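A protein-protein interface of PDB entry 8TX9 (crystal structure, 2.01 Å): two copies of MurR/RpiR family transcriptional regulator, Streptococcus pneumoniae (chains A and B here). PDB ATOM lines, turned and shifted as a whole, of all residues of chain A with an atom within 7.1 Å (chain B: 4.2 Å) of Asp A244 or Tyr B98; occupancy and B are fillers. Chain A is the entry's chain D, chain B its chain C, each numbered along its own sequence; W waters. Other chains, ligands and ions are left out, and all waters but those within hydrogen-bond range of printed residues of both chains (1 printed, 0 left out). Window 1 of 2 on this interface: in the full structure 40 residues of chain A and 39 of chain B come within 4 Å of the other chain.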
ATOM      1  N   TYR A  98     -11.106  -0.183 -16.236  1.00  0.00           N
ATOM      2  CA  TYR A  98     -10.407   1.109 -16.200  1.00  0.00           C
ATOM      3  C   TYR A  98      -9.087   1.041 -16.960  1.00  0.00           C
ATOM      4  O   TYR A  98      -8.780   1.900 -17.792  1.00  0.00           O
ATOM      5  CB  TYR A  98     -10.192   1.580 -14.754  1.00  0.00           C
ATOM      6  CG  TYR A  98     -11.413   2.298 -14.163  1.00  0.00           C
ATOM      7  CD1 TYR A  98     -12.465   1.596 -13.658  1.00  0.00           C
ATOM      8  CD2 TYR A  98     -11.460   3.669 -14.180  1.00  0.00           C
ATOM      9  CE1 TYR A  98     -13.609   2.266 -13.158  1.00  0.00           C
ATOM     10  CE2 TYR A  98     -12.556   4.354 -13.647  1.00  0.00           C
ATOM     11  CZ  TYR A  98     -13.626   3.640 -13.150  1.00  0.00           C
ATOM     12  OH  TYR A  98     -14.722   4.301 -12.610  1.00  0.00           O
ATOM     13  N   ARG A 102      -7.954   3.174 -20.364  1.00  0.00           N
ATOM     14  CA  ARG A 102      -6.733   3.971 -20.457  1.00  0.00           C
ATOM     15  C   ARG A 102      -5.884   3.529 -21.649  1.00  0.00           C
ATOM     16  O   ARG A 102      -5.477   4.352 -22.469  1.00  0.00           O
ATOM     17  CB  ARG A 102      -5.943   3.840 -19.146  1.00  0.00           C
ATOM     18  CG  ARG A 102      -4.445   4.097 -19.237  1.00  0.00           C
ATOM     19  CD  ARG A 102      -4.235   5.540 -19.376  1.00  0.00           C
ATOM     20  NE  ARG A 102      -2.847   5.948 -19.174  1.00  0.00           N
ATOM     21  CZ  ARG A 102      -1.857   5.711 -20.032  1.00  0.00           C
ATOM     22  NH1 ARG A 102      -2.057   5.038 -21.160  1.00  0.00           N
ATOM     23  NH2 ARG A 102      -0.644   6.190 -19.764  1.00  0.00           N
ATOM     24  N   GLU A 141     -19.871  18.903 -16.487  1.00  0.00           N
ATOM     25  CA  GLU A 141     -18.561  19.082 -15.871  1.00  0.00           C
ATOM     26  C   GLU A 141     -17.676  19.885 -16.787  1.00  0.00           C
ATOM     27  O   GLU A 141     -16.823  20.618 -16.317  1.00  0.00           O
ATOM     28  CB  GLU A 141     -17.821  17.790 -15.497  1.00  0.00           C
ATOM     29  CG  GLU A 141     -16.957  18.091 -14.211  1.00  0.00           C
ATOM     30  CD  GLU A 141     -15.824  17.153 -13.874  1.00  0.00           C
ATOM     31  OE1 GLU A 141     -15.597  16.168 -14.598  1.00  0.00           O
ATOM     32  OE2 GLU A 141     -15.095  17.438 -12.857  1.00  0.00           O
ATOM     33  N   MET A 142     -17.829  19.736 -18.104  1.00  0.00           N
ATOM     34  CA  MET A 142     -16.974  20.518 -18.982  1.00  0.00           C
ATOM     35  C   MET A 142     -17.278  22.008 -18.763  1.00  0.00           C
ATOM     36  O   MET A 142     -16.355  22.830 -18.627  1.00  0.00           O
ATOM     37  CB  MET A 142     -17.148  20.077 -20.432  1.00  0.00           C
ATOM     38  CG  MET A 142     -15.862  20.273 -21.190  1.00  0.00           C
ATOM     39  SD  MET A 142     -15.905  19.664 -22.868  1.00  0.00           S
ATOM     40  CE  MET A 142     -14.376  20.399 -23.463  1.00  0.00           C
ATOM     41  N   ARG A 145     -15.562  23.342 -15.543  1.00  0.00           N
ATOM     42  CA  ARG A 145     -14.092  23.467 -15.610  1.00  0.00           C
ATOM     43  C   ARG A 145     -13.668  24.579 -16.570  1.00  0.00           C
ATOM     44  O   ARG A 145     -12.764  25.330 -16.216  1.00  0.00           O
ATOM     45  CB  ARG A 145     -13.522  22.098 -15.958  1.00  0.00           C
ATOM     46  CG  ARG A 145     -13.795  21.069 -14.871  1.00  0.00           C
ATOM     47  CD  ARG A 145     -13.192  19.745 -15.232  1.00  0.00           C
ATOM     48  NE  ARG A 145     -11.751  19.803 -15.042  1.00  0.00           N
ATOM     49  CZ  ARG A 145     -10.913  18.922 -15.548  1.00  0.00           C
ATOM     50  NH1 ARG A 145     -11.374  17.909 -16.254  1.00  0.00           N
ATOM     51  NH2 ARG A 145      -9.612  19.054 -15.338  1.00  0.00           N
ATOM     52  N   PHE A 146     -14.307  24.704 -17.732  1.00  0.00           N
ATOM     53  CA  PHE A 146     -13.888  25.701 -18.695  1.00  0.00           C
ATOM     54  C   PHE A 146     -14.359  27.112 -18.314  1.00  0.00           C
ATOM     55  O   PHE A 146     -13.636  28.078 -18.599  1.00  0.00           O
ATOM     56  CB  PHE A 146     -14.329  25.318 -20.129  1.00  0.00           C
ATOM     57  CG  PHE A 146     -13.401  24.319 -20.816  1.00  0.00           C
ATOM     58  CD1 PHE A 146     -13.402  22.987 -20.446  1.00  0.00           C
ATOM     59  CD2 PHE A 146     -12.489  24.739 -21.771  1.00  0.00           C
ATOM     60  CE1 PHE A 146     -12.469  22.073 -20.989  1.00  0.00           C
ATOM     61  CE2 PHE A 146     -11.612  23.851 -22.365  1.00  0.00           C
ATOM     62  CZ  PHE A 146     -11.573  22.505 -21.937  1.00  0.00           C
ATOM     63  N   LEU A 237     -16.748   7.982 -18.597  1.00  0.00           N
ATOM     64  CA  LEU A 237     -15.292   7.883 -18.583  1.00  0.00           C
ATOM     65  C   LEU A 237     -14.631   8.044 -19.937  1.00  0.00           C
ATOM     66  O   LEU A 237     -13.592   8.730 -20.016  1.00  0.00           O
ATOM     67  CB  LEU A 237     -14.910   6.573 -17.906  1.00  0.00           C
ATOM     68  CG  LEU A 237     -14.579   6.854 -16.421  1.00  0.00           C
ATOM     69  CD1 LEU A 237     -14.762   5.621 -15.534  1.00  0.00           C
ATOM     70  CD2 LEU A 237     -13.157   7.431 -16.326  1.00  0.00           C
ATOM     71  N   PRO A 238     -15.100   7.400 -21.016  1.00  0.00           N
ATOM     72  CA  PRO A 238     -14.458   7.651 -22.308  1.00  0.00           C
ATOM     73  C   PRO A 238     -14.386   9.123 -22.662  1.00  0.00           C
ATOM     74  O   PRO A 238     -13.374   9.557 -23.261  1.00  0.00           O
ATOM     75  CB  PRO A 238     -15.345   6.885 -23.313  1.00  0.00           C
ATOM     76  CG  PRO A 238     -16.063   5.857 -22.513  1.00  0.00           C
ATOM     77  CD  PRO A 238     -16.184   6.401 -21.090  1.00  0.00           C
ATOM     78  N   MET A 239     -15.428   9.881 -22.294  1.00  0.00           N
ATOM     79  CA  MET A 239     -15.458  11.322 -22.578  1.00  0.00           C
ATOM     80  C   MET A 239     -14.513  12.115 -21.649  1.00  0.00           C
ATOM     81  O   MET A 239     -13.807  13.016 -22.112  1.00  0.00           O
ATOM     82  CB  MET A 239     -16.877  11.914 -22.388  1.00  0.00           C
ATOM     83  CG  MET A 239     -18.007  11.431 -23.349  1.00  0.00           C
ATOM     84  SD  MET A 239     -17.389  11.203 -24.988  1.00  0.00           S
ATOM     85  CE  MET A 239     -18.976  10.693 -25.660  1.00  0.00           C
ATOM     86  N   LEU A 240     -14.457  11.748 -20.383  1.00  0.00           N
ATOM     87  CA  LEU A 240     -13.634  12.504 -19.435  1.00  0.00           C
ATOM     88  C   LEU A 240     -12.180  12.441 -19.831  1.00  0.00           C
ATOM     89  O   LEU A 240     -11.486  13.458 -19.799  1.00  0.00           O
ATOM     90  CB  LEU A 240     -13.825  11.963 -18.032  1.00  0.00           C
ATOM     91  CG  LEU A 240     -15.225  12.174 -17.403  1.00  0.00           C
ATOM     92  CD1 LEU A 240     -15.439  11.528 -16.022  1.00  0.00           C
ATOM     93  CD2 LEU A 240     -15.455  13.665 -17.272  1.00  0.00           C
ATOM     94  N   PHE A 241     -11.712  11.283 -20.294  1.00  0.00           N
ATOM     95  CA  PHE A 241     -10.346  11.221 -20.831  1.00  0.00           C
ATOM     96  C   PHE A 241     -10.096  12.317 -21.826  1.00  0.00           C
ATOM     97  O   PHE A 241      -9.094  13.019 -21.764  1.00  0.00           O
ATOM     98  CB  PHE A 241     -10.119   9.879 -21.557  1.00  0.00           C
ATOM     99  CG  PHE A 241      -9.627   8.848 -20.684  1.00  0.00           C
ATOM    100  CD1 PHE A 241      -8.315   8.829 -20.328  1.00  0.00           C
ATOM    101  CD2 PHE A 241     -10.449   7.873 -20.228  1.00  0.00           C
ATOM    102  CE1 PHE A 241      -7.840   7.856 -19.551  1.00  0.00           C
ATOM    103  CE2 PHE A 241      -9.989   6.872 -19.449  1.00  0.00           C
ATOM    104  CZ  PHE A 241      -8.673   6.858 -19.112  1.00  0.00           C
ATOM    105  N   PHE A 242     -10.994  12.459 -22.806  1.00  0.00           N
ATOM    106  CA  PHE A 242     -10.684  13.377 -23.862  1.00  0.00           C
ATOM    107  C   PHE A 242     -10.920  14.815 -23.419  1.00  0.00           C
ATOM    108  O   PHE A 242     -10.179  15.706 -23.803  1.00  0.00           O
ATOM    109  CB  PHE A 242     -11.444  13.001 -25.104  1.00  0.00           C
ATOM    110  CG  PHE A 242     -10.739  11.971 -25.869  1.00  0.00           C
ATOM    111  CD1 PHE A 242     -10.934  10.639 -25.593  1.00  0.00           C
ATOM    112  CD2 PHE A 242      -9.813  12.351 -26.803  1.00  0.00           C
ATOM    113  CE1 PHE A 242     -10.252   9.713 -26.303  1.00  0.00           C
ATOM    114  CE2 PHE A 242      -9.076  11.427 -27.452  1.00  0.00           C
ATOM    115  CZ  PHE A 242      -9.300  10.103 -27.197  1.00  0.00           C
ATOM    116  N   ILE A 243     -11.897  15.026 -22.553  1.00  0.00           N
ATOM    117  CA  ILE A 243     -12.091  16.362 -22.017  1.00  0.00           C
ATOM    118  C   ILE A 243     -10.841  16.813 -21.252  1.00  0.00           C
ATOM    119  O   ILE A 243     -10.428  17.965 -21.348  1.00  0.00           O
ATOM    120  CB  ILE A 243     -13.330  16.417 -21.115  1.00  0.00           C
ATOM    121  CG1 ILE A 243     -14.597  16.355 -21.962  1.00  0.00           C
ATOM    122  CG2 ILE A 243     -13.278  17.651 -20.219  1.00  0.00           C
ATOM    123  CD1 ILE A 243     -15.747  15.881 -21.136  1.00  0.00           C
ATOM    124  N   ASP A 244     -10.292  15.942 -20.407  1.00  0.00           N
ATOM    125  CA  ASP A 244      -9.080  16.296 -19.669  1.00  0.00           C
ATOM    126  C   ASP A 244      -7.897  16.570 -20.613  1.00  0.00           C
ATOM    127  O   ASP A 244      -7.042  17.446 -20.353  1.00  0.00           O
ATOM    128  CB  ASP A 244      -8.762  15.199 -18.673  1.00  0.00           C
ATOM    129  CG  ASP A 244      -9.328  15.475 -17.325  1.00  0.00           C
ATOM    130  OD1 ASP A 244      -9.172  16.643 -16.847  1.00  0.00           O
ATOM    131  OD2 ASP A 244      -9.895  14.521 -16.744  1.00  0.00           O
ATOM    132  N   LEU A 245      -7.795  15.809 -21.701  1.00  0.00           N
ATOM    133  CA  LEU A 245      -6.768  16.105 -22.692  1.00  0.00           C
ATOM    134  C   LEU A 245      -6.968  17.487 -23.281  1.00  0.00           C
ATOM    135  O   LEU A 245      -6.017  18.277 -23.388  1.00  0.00           O
ATOM    136  CB  LEU A 245      -6.788  15.035 -23.786  1.00  0.00           C
ATOM    137  CG  LEU A 245      -6.242  13.684 -23.319  1.00  0.00           C
ATOM    138  CD1 LEU A 245      -6.569  12.617 -24.359  1.00  0.00           C
ATOM    139  CD2 LEU A 245      -4.766  13.808 -23.082  1.00  0.00           C
ATOM    140  N   ILE A 246      -8.194  17.795 -23.691  1.00  0.00           N
ATOM    141  CA  ILE A 246      -8.439  19.107 -24.271  1.00  0.00           C
ATOM    142  C   ILE A 246      -8.175  20.214 -23.241  1.00  0.00           C
ATOM    143  O   ILE A 246      -7.496  21.211 -23.538  1.00  0.00           O
ATOM    144  CB  ILE A 246      -9.864  19.138 -24.845  1.00  0.00           C
ATOM    145  CG1 ILE A 246      -9.922  18.168 -26.047  1.00  0.00           C
ATOM    146  CG2 ILE A 246     -10.233  20.514 -25.228  1.00  0.00           C
ATOM    147  CD1 ILE A 246     -11.379  17.782 -26.504  1.00  0.00           C
ATOM    148  N   TYR A 247      -8.617  20.009 -22.002  1.00  0.00           N
ATOM    149  CA  TYR A 247      -8.404  20.997 -20.959  1.00  0.00           C
ATOM    150  C   TYR A 247      -6.926  21.397 -20.861  1.00  0.00           C
ATOM    151  O   TYR A 247      -6.588  22.579 -20.868  1.00  0.00           O
ATOM    152  CB  TYR A 247      -8.865  20.412 -19.624  1.00  0.00           C
ATOM    153  CG  TYR A 247      -8.700  21.342 -18.409  1.00  0.00           C
ATOM    154  CD1 TYR A 247      -9.606  22.331 -18.131  1.00  0.00           C
ATOM    155  CD2 TYR A 247      -7.632  21.154 -17.534  1.00  0.00           C
ATOM    156  CE1 TYR A 247      -9.409  23.183 -17.034  1.00  0.00           C
ATOM    157  CE2 TYR A 247      -7.491  21.928 -16.417  1.00  0.00           C
ATOM    158  CZ  TYR A 247      -8.359  22.960 -16.197  1.00  0.00           C
ATOM    159  OH  TYR A 247      -8.149  23.715 -15.084  1.00  0.00           O
ATOM    160  N   ALA A 248      -6.053  20.415 -20.771  1.00  0.00           N
ATOM    161  CA  ALA A 248      -4.618  20.685 -20.608  1.00  0.00           C
ATOM    162  C   ALA A 248      -4.032  21.483 -21.764  1.00  0.00           C
ATOM    163  O   ALA A 248      -3.265  22.443 -21.537  1.00  0.00           O
ATOM    164  CB  ALA A 248      -3.861  19.385 -20.446  1.00  0.00           C
ATOM    165  N   TYR A 249      -4.389  21.110 -23.010  1.00  0.00           N
ATOM    166  CA  TYR A 249      -4.001  21.861 -24.199  1.00  0.00           C
ATOM    167  C   TYR A 249      -4.504  23.298 -24.142  1.00  0.00           C
ATOM    168  O   TYR A 249      -3.784  24.228 -24.515  1.00  0.00           O
ATOM    169  CB  TYR A 249      -4.530  21.162 -25.467  1.00  0.00           C
ATOM    170  CG  TYR A 249      -3.710  19.946 -25.834  1.00  0.00           C
ATOM    171  CD1 TYR A 249      -3.473  18.941 -24.928  1.00  0.00           C
ATOM    172  CD2 TYR A 249      -3.088  19.860 -27.074  1.00  0.00           C
ATOM    173  CE1 TYR A 249      -2.682  17.844 -25.250  1.00  0.00           C
ATOM    174  CE2 TYR A 249      -2.284  18.766 -27.408  1.00  0.00           C
ATOM    175  CZ  TYR A 249      -2.091  17.767 -26.483  1.00  0.00           C
ATOM    176  OH  TYR A 249      -1.307  16.681 -26.777  1.00  0.00           O
ATOM    177  N   PHE A 250      -5.745  23.474 -23.688  1.00  0.00           N
ATOM    178  CA  PHE A 250      -6.408  24.761 -23.669  1.00  0.00           C
ATOM    179  C   PHE A 250      -5.825  25.656 -22.578  1.00  0.00           C
ATOM    180  O   PHE A 250      -5.869  26.885 -22.688  1.00  0.00           O
ATOM    181  CB  PHE A 250      -7.878  24.561 -23.414  1.00  0.00           C
ATOM    182  CG  PHE A 250      -8.625  25.823 -23.224  1.00  0.00           C
ATOM    183  CD1 PHE A 250      -9.131  26.498 -24.318  1.00  0.00           C
ATOM    184  CD2 PHE A 250      -8.965  26.256 -21.942  1.00  0.00           C
ATOM    185  CE1 PHE A 250      -9.883  27.647 -24.153  1.00  0.00           C
ATOM    186  CE2 PHE A 250      -9.700  27.394 -21.757  1.00  0.00           C
ATOM    187  CZ  PHE A 250     -10.138  28.138 -22.873  1.00  0.00           C
ATOM    188  N   VAL B  94      -1.344  14.130 -18.603  1.00  0.00           N
ATOM    189  CA  VAL B  94      -2.758  13.742 -18.358  1.00  0.00           C
ATOM    190  C   VAL B  94      -2.878  12.233 -18.186  1.00  0.00           C
ATOM    191  O   VAL B  94      -3.485  11.720 -17.239  1.00  0.00           O
ATOM    192  CB  VAL B  94      -3.654  14.224 -19.504  1.00  0.00           C
ATOM    193  CG1 VAL B  94      -5.061  13.599 -19.370  1.00  0.00           C
ATOM    194  CG2 VAL B  94      -3.678  15.719 -19.530  1.00  0.00           C
ATOM    195  N   LEU B  95      -2.297  11.485 -19.122  1.00  0.00           N
ATOM    196  CA  LEU B  95      -2.363  10.035 -19.044  1.00  0.00           C
ATOM    197  C   LEU B  95      -1.708   9.513 -17.782  1.00  0.00           C
ATOM    198  O   LEU B  95      -2.171   8.531 -17.188  1.00  0.00           O
ATOM    199  CB  LEU B  95      -1.727   9.450 -20.303  1.00  0.00           C
ATOM    200  CG  LEU B  95      -2.549   9.726 -21.571  1.00  0.00           C
ATOM    201  CD1 LEU B  95      -1.840   9.224 -22.834  1.00  0.00           C
ATOM    202  CD2 LEU B  95      -3.951   9.109 -21.495  1.00  0.00           C
ATOM    203  N   ARG B  96      -0.590  10.143 -17.363  1.00  0.00           N
ATOM    204  CA  ARG B  96       0.030   9.712 -16.116  1.00  0.00           C
ATOM    205  C   ARG B  96      -0.918   9.921 -14.939  1.00  0.00           C
ATOM    206  O   ARG B  96      -0.987   9.078 -14.029  1.00  0.00           O
ATOM    207  CB  ARG B  96       1.379  10.462 -15.901  1.00  0.00           C
ATOM    208  CG  ARG B  96       2.313   9.902 -14.746  1.00  0.00           C
ATOM    209  CD  ARG B  96       3.748  10.561 -14.764  1.00  0.00           C
ATOM    210  NE  ARG B  96       4.097  11.072 -16.088  1.00  0.00           N
ATOM    211  CZ  ARG B  96       4.158  12.361 -16.396  1.00  0.00           C
ATOM    212  NH1 ARG B  96       3.844  13.288 -15.537  1.00  0.00           N
ATOM    213  NH2 ARG B  96       4.523  12.722 -17.632  1.00  0.00           N
ATOM    214  N   SER B  97      -1.628  11.050 -14.907  1.00  0.00           N
ATOM    215  CA  SER B  97      -2.623  11.295 -13.833  1.00  0.00           C
ATOM    216  C   SER B  97      -3.657  10.172 -13.760  1.00  0.00           C
ATOM    217  O   SER B  97      -3.986   9.687 -12.672  1.00  0.00           O
ATOM    218  CB  SER B  97      -3.365  12.604 -14.055  1.00  0.00           C
ATOM    219  OG  SER B  97      -2.545  13.756 -13.894  1.00  0.00           O
ATOM    220  N   TYR B  98      -4.092   9.692 -14.915  1.00  0.00           N
ATOM    221  CA  TYR B  98      -5.095   8.618 -14.921  1.00  0.00           C
ATOM    222  C   TYR B  98      -4.480   7.323 -14.433  1.00  0.00           C
ATOM    223  O   TYR B  98      -5.053   6.623 -13.583  1.00  0.00           O
ATOM    224  CB  TYR B  98      -5.737   8.425 -16.292  1.00  0.00           C
ATOM    225  CG  TYR B  98      -6.879   9.383 -16.627  1.00  0.00           C
ATOM    226  CD1 TYR B  98      -6.668  10.681 -17.015  1.00  0.00           C
ATOM    227  CD2 TYR B  98      -8.183   8.927 -16.545  1.00  0.00           C
ATOM    228  CE1 TYR B  98      -7.762  11.556 -17.307  1.00  0.00           C
ATOM    229  CE2 TYR B  98      -9.263   9.744 -16.876  1.00  0.00           C
ATOM    230  CZ  TYR B  98      -9.065  11.063 -17.202  1.00  0.00           C
ATOM    231  OH  TYR B  98     -10.187  11.835 -17.468  1.00  0.00           O
ATOM    232  N   SER B  99      -3.270   6.991 -14.932  1.00  0.00           N
ATOM    233  CA  SER B  99      -2.572   5.778 -14.449  1.00  0.00           C
ATOM    234  C   SER B  99      -2.313   5.815 -12.959  1.00  0.00           C
ATOM    235  O   SER B  99      -2.528   4.822 -12.245  1.00  0.00           O
ATOM    236  CB  SER B  99      -1.225   5.656 -15.173  1.00  0.00           C
ATOM    237  OG  SER B  99      -1.476   5.631 -16.540  1.00  0.00           O
ATOM    238  N   ASN B 100      -1.794   6.945 -12.467  1.00  0.00           N
ATOM    239  CA  ASN B 100      -1.501   7.054 -11.029  1.00  0.00           C
ATOM    240  C   ASN B 100      -2.750   6.893 -10.205  1.00  0.00           C
ATOM    241  O   ASN B 100      -2.726   6.305  -9.117  1.00  0.00           O
ATOM    242  CB  ASN B 100      -0.866   8.406 -10.685  1.00  0.00           C
ATOM    243  CG  ASN B 100       0.455   8.602 -11.380  1.00  0.00           C
ATOM    244  OD1 ASN B 100       1.089   7.635 -11.813  1.00  0.00           O
ATOM    245  ND2 ASN B 100       0.872   9.853 -11.482  1.00  0.00           N
ATOM    246  N   MET B 101      -3.863   7.465 -10.681  1.00  0.00           N
ATOM    247  CA  MET B 101      -5.103   7.290  -9.944  1.00  0.00           C
ATOM    248  C   MET B 101      -5.569   5.845  -9.899  1.00  0.00           C
ATOM    249  O   MET B 101      -6.052   5.356  -8.904  1.00  0.00           O
ATOM    250  CB  MET B 101      -6.178   8.204 -10.521  1.00  0.00           C
ATOM    251  CG  MET B 101      -7.246   8.451  -9.502  1.00  0.00           C
ATOM    252  SD  MET B 101      -8.330   9.751 -10.022  1.00  0.00           S
ATOM    253  CE  MET B 101      -7.378  11.219  -9.584  1.00  0.00           C
ATOM    254  N   ARG B 102      -5.484   5.221 -10.775  1.00  0.00           N
ATOM    255  CA  ARG B 102      -5.844   3.811 -10.884  1.00  0.00           C
ATOM    256  C   ARG B 102      -4.926   2.956 -10.033  1.00  0.00           C
ATOM    257  O   ARG B 102      -5.429   2.093  -9.361  1.00  0.00           O
ATOM    258  CB  ARG B 102      -5.737   3.379 -12.355  1.00  0.00           C
ATOM    259  CG  ARG B 102      -6.635   2.193 -12.692  1.00  0.00           C
ATOM    260  CD  ARG B 102      -5.858   1.025 -13.241  1.00  0.00           C
ATOM    261  NE  ARG B 102      -6.417  -0.239 -12.790  1.00  0.00           N
ATOM    262  CZ  ARG B 102      -5.815  -1.026 -11.909  1.00  0.00           C
ATOM    263  NH1 ARG B 102      -5.492  -0.559 -10.719  1.00  0.00           N
ATOM    264  NH2 ARG B 102      -5.558  -2.286 -12.210  1.00  0.00           N
ATOM    265  N   ILE B 233      -6.742  16.520 -13.082  1.00  0.00           N
ATOM    266  CA  ILE B 233      -7.718  15.938 -13.969  1.00  0.00           C
ATOM    267  C   ILE B 233      -9.043  15.966 -13.193  1.00  0.00           C
ATOM    268  O   ILE B 233      -9.132  16.454 -12.026  1.00  0.00           O
ATOM    269  CB  ILE B 233      -7.301  14.542 -14.441  1.00  0.00           C
ATOM    270  CG1 ILE B 233      -7.206  13.541 -13.302  1.00  0.00           C
ATOM    271  CG2 ILE B 233      -6.038  14.650 -15.209  1.00  0.00           C
ATOM    272  CD1 ILE B 233      -7.110  12.116 -13.777  1.00  0.00           C
ATOM    273  N   SER B 234     -10.089  15.488 -13.840  1.00  0.00           N
ATOM    274  CA  SER B 234     -11.456  15.683 -13.319  1.00  0.00           C
ATOM    275  C   SER B 234     -11.603  15.235 -11.879  1.00  0.00           C
ATOM    276  O   SER B 234     -11.147  14.125 -11.469  1.00  0.00           O
ATOM    277  CB  SER B 234     -12.438  14.894 -14.211  1.00  0.00           C
ATOM    278  OG  SER B 234     -13.685  14.723 -13.540  1.00  0.00           O
ATOM    279  N   LEU B 237     -13.181  11.695 -10.750  1.00  0.00           N
ATOM    280  CA  LEU B 237     -12.577  10.388 -11.063  1.00  0.00           C
ATOM    281  C   LEU B 237     -12.308   9.565  -9.828  1.00  0.00           C
ATOM    282  O   LEU B 237     -12.692   8.383  -9.787  1.00  0.00           O
ATOM    283  CB  LEU B 237     -11.323  10.653 -11.883  1.00  0.00           C
ATOM    284  CG  LEU B 237     -11.558  10.649 -13.378  1.00  0.00           C
ATOM    285  CD1 LEU B 237     -10.475  11.507 -14.113  1.00  0.00           C
ATOM    286  CD2 LEU B 237     -11.619   9.242 -14.040  1.00  0.00           C
HETATM  287  O   HOH W   1       0.911   7.343 -18.150  1.00  0.00           O
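O of Leu B95 lies within hydrogen-bond range of NE of Arg A102 (3.3 Å). OH of Tyr B98 is in hydrogen-bond range of O of Leu A240, at 3.1 Å. The side-chain hydroxyl of Tyr B98 lies within hydrogen-bond range of the backbone NH of Phe A241, 3.3 Å away. OH of Tyr B98 lies within hydrogen-bond range of OD2 of Asp A244. NE of Arg A102 lies within hydrogen-bond range of OG of Ser B99 (3.0 Å). The side-chain hydroxyl (OG) of Ser B234 is in hydrogen-bond range of the side-chain carboxylate (OE1) of Glu A141 (2.6 Å). OD2 of Asp A244 sits at hydrogen-bond distance from N of Ser B234.
O of Leu B95 sits at hydrogen-bond distance from OG of Ser B99, at 3.1 Å. The side-chain carboxylate of Asp A244 lies within salt-bridge range of the guanidinium group of Arg A145, 2.6 Å away.
C of Ile B233 touches NH2 of Arg A145, 3.8 Å away. Arg A145 touches Ser B234 (NH1 to N, 3.7 Å). Leu A237 touches Leu B237 (CD2 to CD2, 3.3 Å). CG2 of Val B94 touches O of Asp A244, at 3.9 Å. Asp A244 touches Ile B233 (OD1 to CA, 3.3 Å). Val B94 touches Leu A245 (CG1 to CD2, 3.7 Å). Val B94 touches Ala A248.
Ile A243 touches none of the printed residues of chain B. Of chain B, only Val B94 (3.9 Å), Tyr B98 (2.8 Å), Ile B233 (3.3 Å) and Ser B234 (3.1 Å) come within 4 Å of Asp A244. Of the printed residues of chain B, Ala A248 touches Val B94 (3.8 Å). Tyr B98 touches just these residues of chain A: Leu A240 (3.1 Å), Phe A241 (3.2 Å) and Asp A244 (2.8 Å). Asn B100 touches none of the printed residues of chain A. Of the printed residues of chain A, Ile B233 touches Arg A145 (3.8 Å) and Asp A244 (3.3 Å). The nearest residue of chain B that does not touch Asp A244 is Leu B237 (4.04 Å). The nearest residue of chain A that does not touch Tyr B98 is Arg A102 (4.5 Å).
Of the 20 printed residues of chain A, 9 touch a printed residue of chain B. Hydrophobic or aromatic side chains of chain B within 4 Å of the printed part of chain A: Val B94, Leu B95, Tyr B98, Ile B233 and Leu B237. Among the printed residues, 14 pairs touch across the chains. Among the printed residues, no Asp or Glu carboxylate lies within 4 Å of a Lys or Arg side-chain nitrogen of the other chain.
Leu B237 touches its own counterpart, Leu A237. 3 positions are printed for both chains.
Water W1 lies within hydrogen-bond range of the guanidinium group (NH2) of Arg A102 (2.5 Å), the backbone NH (N) of Arg B96 (3.3 Å), the side-chain hydroxyl (OG) of Ser B99 (3.3 Å) and the backbone carbonyl oxygen (O) of Leu B95 (3.4 Å).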
